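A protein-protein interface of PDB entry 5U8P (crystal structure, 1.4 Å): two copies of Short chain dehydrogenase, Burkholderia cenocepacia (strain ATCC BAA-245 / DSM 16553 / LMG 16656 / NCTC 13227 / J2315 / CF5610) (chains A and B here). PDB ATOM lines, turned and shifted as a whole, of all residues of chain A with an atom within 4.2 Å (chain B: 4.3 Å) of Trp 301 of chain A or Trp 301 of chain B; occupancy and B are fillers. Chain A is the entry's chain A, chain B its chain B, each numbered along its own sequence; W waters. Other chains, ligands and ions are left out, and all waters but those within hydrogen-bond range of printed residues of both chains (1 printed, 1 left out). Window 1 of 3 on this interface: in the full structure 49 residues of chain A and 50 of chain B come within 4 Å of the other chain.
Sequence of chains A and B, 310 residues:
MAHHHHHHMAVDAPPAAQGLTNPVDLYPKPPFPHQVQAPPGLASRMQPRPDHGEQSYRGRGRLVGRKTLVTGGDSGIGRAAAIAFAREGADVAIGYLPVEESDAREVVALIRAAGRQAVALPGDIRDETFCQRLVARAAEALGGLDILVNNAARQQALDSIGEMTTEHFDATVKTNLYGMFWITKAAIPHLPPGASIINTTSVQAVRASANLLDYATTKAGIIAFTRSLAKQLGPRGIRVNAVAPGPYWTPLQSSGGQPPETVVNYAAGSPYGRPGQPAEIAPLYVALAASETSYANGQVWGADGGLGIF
Leu 284 of chain A touches Thr 293 of chain B.
CZ2 of Trp 301 of chain B touches CG of Leu 284 of chain A, 3.5 Å away.
Thr 293 of chain A touches Leu 284 of chain B (CG2 to CD1, 3.9 Å).
Gln 299 of chain A touches Gly 302 of chain B.
Ala 303 of chain B touches Gln 299 of chain A.
Trp 301 of chain A touches Leu 284 of chain B (CZ2 to CG, 3.5 Å).
CE3 of Trp 301 of chain A touches CE3 of Trp 301 of chain B (3.7 Å).
Gly 302 of chain A touches Gln 299 of chain B.
Gln 299 of chain B touches Ala 303 of chain A.
The indole nitrogen (NE1) of Trp 301 of chain A lies within hydrogen-bond range of the backbone carbonyl oxygen (O) of Gly 302 of chain B (3.0 Å).
The backbone carbonyl oxygen (O) of Gly 302 of chain A lies within hydrogen-bond range of the indole nitrogen (NE1) of Trp 301 of chain B, 2.9 Å away.
Water W1 lies within hydrogen-bond range of O of Val 300 of chain B (3.0 Å) and O of Val 300 of chain A (3.0 Å).
Ala 244 of chain A touches none of the printed residues of chain B.
Of the printed residues of chain B, Thr 293 of chain A touches Leu 284 (3.9 Å).
Val 300 of chain A touches none of the printed residues of chain B.
Trp 301 of chain A touches three residues of chain B.
Trp 301 of chain B touches just these residues of chain A: Leu 284 (3.5 Å), Trp 301 (3.7 Å) and Gly 302 (2.9 Å).
Printed residues of chain A within 4 Å of Ala 303 of chain B: Gln 299.
The nearest printed residue of chain B that does not touch Trp 301 of chain A is Val 300 of chain B (5.1 Å).
The nearest printed residue of chain A that does not touch Trp 301 of chain B is Val 300 of chain A (5.1 Å).
The nearest printed residue of chain A that does not touch Gln 299 of chain B is Ala 244 of chain A (5.6 Å).
Leu 284 of chain A touches Thr 293 of chain B, and with the chains exchanged Thr 293 of chain A touches Leu 284 of chain B.
Leu 284 of chain A touches Trp 301 of chain B, and with the chains exchanged Trp 301 of chain A touches Leu 284 of chain B.
Trp 301 of chain A touches its own counterpart, Trp 301 of chain B.
Trp 301 of chain A touches Gly 302 of chain B, and with the chains exchanged Gly 302 of chain A touches Trp 301 of chain B.
The backbone carbonyl oxygen (O) of Ala 242 of chain A is in hydrogen-bond range of the backbone NH (N) of Trp 301 of chain A (2.9 Å).
The side-chain hydroxyl (OG1) of Thr 293 of chain A is in hydrogen-bond range of the backbone carbonyl oxygen (O) of Ala 287 of chain A (2.7 Å).
N of Ala 242 of chain B sits at hydrogen-bond distance from O of Gln 299 of chain B (2.8 Å).
The backbone NH (N) of Ala 244 of chain B lies within hydrogen-bond range of the backbone carbonyl oxygen (O) of Trp 301 of chain B, at 2.9 Å.
The backbone carbonyl oxygen of Ala 244 of chain B lies within hydrogen-bond range of the backbone NH of Ala 303 of chain B.
The backbone carbonyl oxygen (O) of Ala 287 of chain B is in hydrogen-bond range of the side-chain hydroxyl (OG1) of Thr 293 of chain B, 2.7 Å away.
Hydrophobic or aromatic side chains of chain A that line the printed part of chain B: Leu 284 and Trp 301.
Of the 13 printed residues of chain B, 6 touch a printed residue of chain A.
Printed residues of chain B that touch a printed residue of chain A: Leu 284, Thr 293, Gln 299, Trp 301, Gly 302 and Ala 303.
Among the printed residues, 11 pairs touch across the chains.
Among the printed residues, no Asp or Glu carboxylate lies within 4 Å of a Lys or Arg side-chain nitrogen of the other chain.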
ATOM      1  N   ALA A 242      13.435  31.402  31.446  1.00  0.00           N
ATOM      2  CA  ALA A 242      12.520  30.719  32.349  1.00  0.00           C
ATOM      3  C   ALA A 242      12.173  29.331  31.818  1.00  0.00           C
ATOM      4  O   ALA A 242      12.198  29.081  30.608  1.00  0.00           O
ATOM      5  CB  ALA A 242      11.215  31.526  32.563  1.00  0.00           C
ATOM      6  N   VAL A 243      11.855  28.425  32.743  1.00  0.00           N
ATOM      7  CA  VAL A 243      11.362  27.085  32.426  1.00  0.00           C
ATOM      8  C   VAL A 243       9.929  26.986  32.937  1.00  0.00           C
ATOM      9  O   VAL A 243       9.657  27.343  34.091  1.00  0.00           O
ATOM     10  CB  VAL A 243      12.251  26.001  33.065  1.00  0.00           C
ATOM     11  CG1 VAL A 243      11.582  24.609  32.955  1.00  0.00           C
ATOM     12  CG2 VAL A 243      13.646  25.999  32.429  1.00  0.00           C
ATOM     13  N   ALA A 244       9.014  26.493  32.085  1.00  0.00           N
ATOM     14  CA  ALA A 244       7.592  26.355  32.424  1.00  0.00           C
ATOM     15  C   ALA A 244       7.191  24.879  32.505  1.00  0.00           C
ATOM     16  O   ALA A 244       6.724  24.298  31.511  1.00  0.00           O
ATOM     17  CB  ALA A 244       6.732  27.101  31.401  1.00  0.00           C
ATOM     18  N   LEU A 284      16.448  20.721  30.322  1.00  0.00           N
ATOM     19  CA  LEU A 284      16.172  22.109  29.943  1.00  0.00           C
ATOM     20  C   LEU A 284      17.088  23.072  30.678  1.00  0.00           C
ATOM     21  O   LEU A 284      17.569  24.053  30.090  1.00  0.00           O
ATOM     22  CB  LEU A 284      14.717  22.481  30.247  1.00  0.00           C
ATOM     23  CG  LEU A 284      13.654  22.085  29.216  1.00  0.00           C
ATOM     24  CD1 LEU A 284      13.443  20.561  29.150  1.00  0.00           C
ATOM     25  CD2 LEU A 284      12.342  22.810  29.510  1.00  0.00           C
ATOM     26  N   ALA A 287      20.619  22.793  29.172  1.00  0.00           N
ATOM     27  CA  ALA A 287      20.696  23.443  27.865  1.00  0.00           C
ATOM     28  C   ALA A 287      20.665  24.963  27.997  1.00  0.00           C
ATOM     29  O   ALA A 287      21.430  25.668  27.325  1.00  0.00           O
ATOM     30  CB  ALA A 287      19.583  22.948  26.947  1.00  0.00           C
ATOM     31  N   LEU A 288      19.800  25.495  28.868  1.00  0.00           N
ATOM     32  CA  LEU A 288      19.738  26.952  28.991  1.00  0.00           C
ATOM     33  C   LEU A 288      21.026  27.519  29.567  1.00  0.00           C
ATOM     34  O   LEU A 288      21.436  28.620  29.173  1.00  0.00           O
ATOM     35  CB  LEU A 288      18.541  27.384  29.832  1.00  0.00           C
ATOM     36  CG  LEU A 288      17.197  27.295  29.104  1.00  0.00           C
ATOM     37  CD1 LEU A 288      16.055  27.421  30.103  1.00  0.00           C
ATOM     38  CD2 LEU A 288      17.078  28.338  27.987  1.00  0.00           C
ATOM     39  N   THR A 293      24.518  27.800  24.049  1.00  0.00           N
ATOM     40  CA  THR A 293      23.120  28.172  23.778  1.00  0.00           C
ATOM     41  C   THR A 293      22.985  29.700  23.837  1.00  0.00           C
ATOM     42  O   THR A 293      22.169  30.275  24.571  1.00  0.00           O
ATOM     43  CB  THR A 293      22.191  27.459  24.765  1.00  0.00           C
ATOM     44  OG1 THR A 293      22.630  26.100  24.913  1.00  0.00           O
ATOM     45  CG2 THR A 293      20.740  27.447  24.280  1.00  0.00           C
ATOM     46  N   ALA A 296      19.755  32.211  23.236  1.00  0.00           N
ATOM     47  CA  ALA A 296      18.542  32.009  24.026  1.00  0.00           C
ATOM     48  C   ALA A 296      18.568  32.996  25.187  1.00  0.00           C
ATOM     49  O   ALA A 296      19.353  32.837  26.131  1.00  0.00           O
ATOM     50  CB  ALA A 296      18.453  30.568  24.534  1.00  0.00           C
ATOM     51  N   GLN A 299      13.678  33.795  27.045  1.00  0.00           N
ATOM     52  CA  GLN A 299      12.758  32.764  26.579  1.00  0.00           C
ATOM     53  C   GLN A 299      12.043  32.098  27.744  1.00  0.00           C
ATOM     54  O   GLN A 299      12.519  32.091  28.882  1.00  0.00           O
ATOM     55  CB  GLN A 299      13.500  31.660  25.810  1.00  0.00           C
ATOM     56  CG  GLN A 299      14.734  32.080  25.011  1.00  0.00           C
ATOM     57  CD  GLN A 299      14.471  33.033  23.849  1.00  0.00           C
ATOM     58  OE1 GLN A 299      15.437  33.528  23.251  1.00  0.00           O
ATOM     59  NE2 GLN A 299      13.190  33.272  23.494  1.00  0.00           N
ATOM     60  N   VAL A 300      10.898  31.490  27.437  1.00  0.00           N
ATOM     61  CA  VAL A 300      10.192  30.604  28.362  1.00  0.00           C
ATOM     62  C   VAL A 300      10.097  29.256  27.662  1.00  0.00           C
ATOM     63  O   VAL A 300       9.352  29.115  26.686  1.00  0.00           O
ATOM     64  CB  VAL A 300       8.787  31.125  28.718  1.00  0.00           C
ATOM     65  CG1 VAL A 300       8.107  30.168  29.703  1.00  0.00           C
ATOM     66  CG2 VAL A 300       8.852  32.558  29.268  1.00  0.00           C
ATOM     67  N   TRP A 301      10.834  28.253  28.149  1.00  0.00           N
ATOM     68  CA  TRP A 301      10.803  26.922  27.540  1.00  0.00           C
ATOM     69  C   TRP A 301       9.916  26.002  28.377  1.00  0.00           C
ATOM     70  O   TRP A 301      10.209  25.746  29.550  1.00  0.00           O
ATOM     71  CB  TRP A 301      12.207  26.318  27.455  1.00  0.00           C
ATOM     72  CG  TRP A 301      13.090  26.937  26.421  1.00  0.00           C
ATOM     73  CD1 TRP A 301      12.815  28.011  25.608  1.00  0.00           C
ATOM     74  CD2 TRP A 301      14.418  26.512  26.092  1.00  0.00           C
ATOM     75  NE1 TRP A 301      13.904  28.272  24.785  1.00  0.00           N
ATOM     76  CE2 TRP A 301      14.893  27.358  25.056  1.00  0.00           C
ATOM     77  CE3 TRP A 301      15.236  25.468  26.544  1.00  0.00           C
ATOM     78  CZ2 TRP A 301      16.159  27.207  24.483  1.00  0.00           C
ATOM     79  CZ3 TRP A 301      16.510  25.322  25.986  1.00  0.00           C
ATOM     80  CH2 TRP A 301      16.952  26.188  24.956  1.00  0.00           C
ATOM     81  N   GLY A 302       8.835  25.477  27.767  1.00  0.00           N
ATOM     82  CA  GLY A 302       7.972  24.555  28.480  1.00  0.00           C
ATOM     83  C   GLY A 302       8.402  23.096  28.411  1.00  0.00           C
ATOM     84  O   GLY A 302       9.117  22.658  27.503  1.00  0.00           O
ATOM     85  N   ALA A 303       7.942  22.333  29.411  1.00  0.00           N
ATOM     86  CA  ALA A 303       8.050  20.870  29.377  1.00  0.00           C
ATOM     87  C   ALA A 303       6.819  20.352  30.127  1.00  0.00           C
ATOM     88  O   ALA A 303       6.854  20.100  31.344  1.00  0.00           O
ATOM     89  CB  ALA A 303       9.362  20.369  29.975  1.00  0.00           C
ATOM     90  N   ALA B 242       8.294  22.594  18.469  1.00  0.00           N
ATOM     91  CA  ALA B 242       8.677  23.627  17.516  1.00  0.00           C
ATOM     92  C   ALA B 242       9.784  24.494  18.107  1.00  0.00           C
ATOM     93  O   ALA B 242       9.917  24.611  19.335  1.00  0.00           O
ATOM     94  CB  ALA B 242       7.468  24.510  17.126  1.00  0.00           C
ATOM     95  N   VAL B 243      10.585  25.085  17.215  1.00  0.00           N
ATOM     96  CA  VAL B 243      11.632  26.040  17.568  1.00  0.00           C
ATOM     97  C   VAL B 243      11.268  27.373  16.930  1.00  0.00           C
ATOM     98  O   VAL B 243      10.941  27.419  15.738  1.00  0.00           O
ATOM     99  CB  VAL B 243      13.006  25.557  17.070  1.00  0.00           C
ATOM    100  CG1 VAL B 243      14.042  26.676  17.183  1.00  0.00           C
ATOM    101  CG2 VAL B 243      13.450  24.322  17.856  1.00  0.00           C
ATOM    102  N   ALA B 244      11.320  28.458  17.715  1.00  0.00           N
ATOM    103  CA  ALA B 244      10.973  29.803  17.251  1.00  0.00           C
ATOM    104  C   ALA B 244      12.207  30.701  17.229  1.00  0.00           C
ATOM    105  O   ALA B 244      12.514  31.373  18.224  1.00  0.00           O
ATOM    106  CB  ALA B 244       9.877  30.410  18.131  1.00  0.00           C
ATOM    107  N   LEU B 284      19.144  23.705  20.541  1.00  0.00           N
ATOM    108  CA  LEU B 284      17.724  23.481  20.815  1.00  0.00           C
ATOM    109  C   LEU B 284      17.220  22.235  20.101  1.00  0.00           C
ATOM    110  O   LEU B 284      16.416  21.472  20.655  1.00  0.00           O
ATOM    111  CB  LEU B 284      16.876  24.682  20.369  1.00  0.00           C
ATOM    112  CG  LEU B 284      16.781  25.898  21.302  1.00  0.00           C
ATOM    113  CD1 LEU B 284      18.146  26.597  21.433  1.00  0.00           C
ATOM    114  CD2 LEU B 284      15.704  26.876  20.820  1.00  0.00           C
ATOM    115  N   ALA B 287      18.582  19.126  21.932  1.00  0.00           N
ATOM    116  CA  ALA B 287      17.885  18.891  23.200  1.00  0.00           C
ATOM    117  C   ALA B 287      16.474  18.357  22.965  1.00  0.00           C
ATOM    118  O   ALA B 287      16.020  17.443  23.671  1.00  0.00           O
ATOM    119  CB  ALA B 287      17.840  20.172  24.035  1.00  0.00           C
ATOM    120  N   LEU B 288      15.751  18.921  21.995  1.00  0.00           N
ATOM    121  CA  LEU B 288      14.386  18.460  21.761  1.00  0.00           C
ATOM    122  C   LEU B 288      14.359  17.031  21.240  1.00  0.00           C
ATOM    123  O   LEU B 288      13.436  16.281  21.567  1.00  0.00           O
ATOM    124  CB  LEU B 288      13.669  19.392  20.789  1.00  0.00           C
ATOM    125  CG  LEU B 288      13.201  20.710  21.413  1.00  0.00           C
ATOM    126  CD1 LEU B 288      12.766  21.652  20.298  1.00  0.00           C
ATOM    127  CD2 LEU B 288      12.057  20.505  22.416  1.00  0.00           C
ATOM    128  N   THR B 293      14.829  14.025  27.043  1.00  0.00           N
ATOM    129  CA  THR B 293      13.960  15.200  27.159  1.00  0.00           C
ATOM    130  C   THR B 293      12.494  14.782  26.999  1.00  0.00           C
ATOM    131  O   THR B 293      11.730  15.288  26.166  1.00  0.00           O
ATOM    132  CB  THR B 293      14.385  16.263  26.144  1.00  0.00           C
ATOM    133  OG1 THR B 293      15.821  16.344  26.101  1.00  0.00           O
ATOM    134  CG2 THR B 293      13.803  17.655  26.495  1.00  0.00           C
ATOM    135  N   ALA B 296       8.997  16.951  27.151  1.00  0.00           N
ATOM    136  CA  ALA B 296       8.836  18.105  26.272  1.00  0.00           C
ATOM    137  C   ALA B 296       8.036  17.645  25.056  1.00  0.00           C
ATOM    138  O   ALA B 296       8.558  16.919  24.199  1.00  0.00           O
ATOM    139  CB  ALA B 296      10.199  18.677  25.874  1.00  0.00           C
ATOM    140  N   GLN B 299       5.717  21.786  22.710  1.00  0.00           N
ATOM    141  CA  GLN B 299       6.317  23.039  23.151  1.00  0.00           C
ATOM    142  C   GLN B 299       6.787  23.862  21.958  1.00  0.00           C
ATOM    143  O   GLN B 299       7.070  23.337  20.872  1.00  0.00           O
ATOM    144  CB  GLN B 299       7.528  22.793  24.068  1.00  0.00           C
ATOM    145  CG  GLN B 299       7.500  21.557  24.948  1.00  0.00           C
ATOM    146  CD  GLN B 299       6.413  21.529  26.016  1.00  0.00           C
ATOM    147  OE1 GLN B 299       6.239  20.491  26.668  1.00  0.00           O
ATOM    148  NE2 GLN B 299       5.714  22.660  26.243  1.00  0.00           N
ATOM    149  N   VAL B 300       6.918  25.174  22.189  1.00  0.00           N
ATOM    150  CA  VAL B 300       7.577  26.093  21.256  1.00  0.00           C
ATOM    151  C   VAL B 300       8.733  26.727  22.024  1.00  0.00           C
ATOM    152  O   VAL B 300       8.506  27.551  22.922  1.00  0.00           O
ATOM    153  CB  VAL B 300       6.627  27.177  20.729  1.00  0.00           C
ATOM    154  CG1 VAL B 300       7.376  28.086  19.741  1.00  0.00           C
ATOM    155  CG2 VAL B 300       5.393  26.539  20.097  1.00  0.00           C
ATOM    156  N   TRP B 301       9.974  26.362  21.674  1.00  0.00           N
ATOM    157  CA  TRP B 301      11.148  26.902  22.358  1.00  0.00           C
ATOM    158  C   TRP B 301      11.759  28.014  21.508  1.00  0.00           C
ATOM    159  O   TRP B 301      12.208  27.768  20.383  1.00  0.00           O
ATOM    160  CB  TRP B 301      12.194  25.816  22.613  1.00  0.00           C
ATOM    161  CG  TRP B 301      11.837  24.834  23.692  1.00  0.00           C
ATOM    162  CD1 TRP B 301      10.663  24.760  24.413  1.00  0.00           C
ATOM    163  CD2 TRP B 301      12.671  23.777  24.164  1.00  0.00           C
ATOM    164  NE1 TRP B 301      10.735  23.715  25.316  1.00  0.00           N
ATOM    165  CE2 TRP B 301      11.963  23.106  25.189  1.00  0.00           C
ATOM    166  CE3 TRP B 301      13.973  23.352  23.847  1.00  0.00           C
ATOM    167  CZ2 TRP B 301      12.496  22.011  25.875  1.00  0.00           C
ATOM    168  CZ3 TRP B 301      14.503  22.271  24.531  1.00  0.00           C
ATOM    169  CH2 TRP B 301      13.765  21.613  25.536  1.00  0.00           C
ATOM    170  N   GLY B 302      11.821  29.236  22.064  1.00  0.00           N
ATOM    171  CA  GLY B 302      12.410  30.346  21.339  1.00  0.00           C
ATOM    172  C   GLY B 302      13.921  30.482  21.518  1.00  0.00           C
ATOM    173  O   GLY B 302      14.513  30.034  22.495  1.00  0.00           O
ATOM    174  N   ALA B 303      14.550  31.122  20.538  1.00  0.00           N
ATOM    175  CA  ALA B 303      15.945  31.545  20.690  1.00  0.00           C
ATOM    176  C   ALA B 303      16.079  32.823  19.857  1.00  0.00           C
ATOM    177  O   ALA B 303      16.418  32.778  18.666  1.00  0.00           O
ATOM    178  CB  ALA B 303      16.943  30.472  20.269  1.00  0.00           C
HETATM  179  O   HOH W   1       7.150  29.515  24.678  1.00  0.00           O
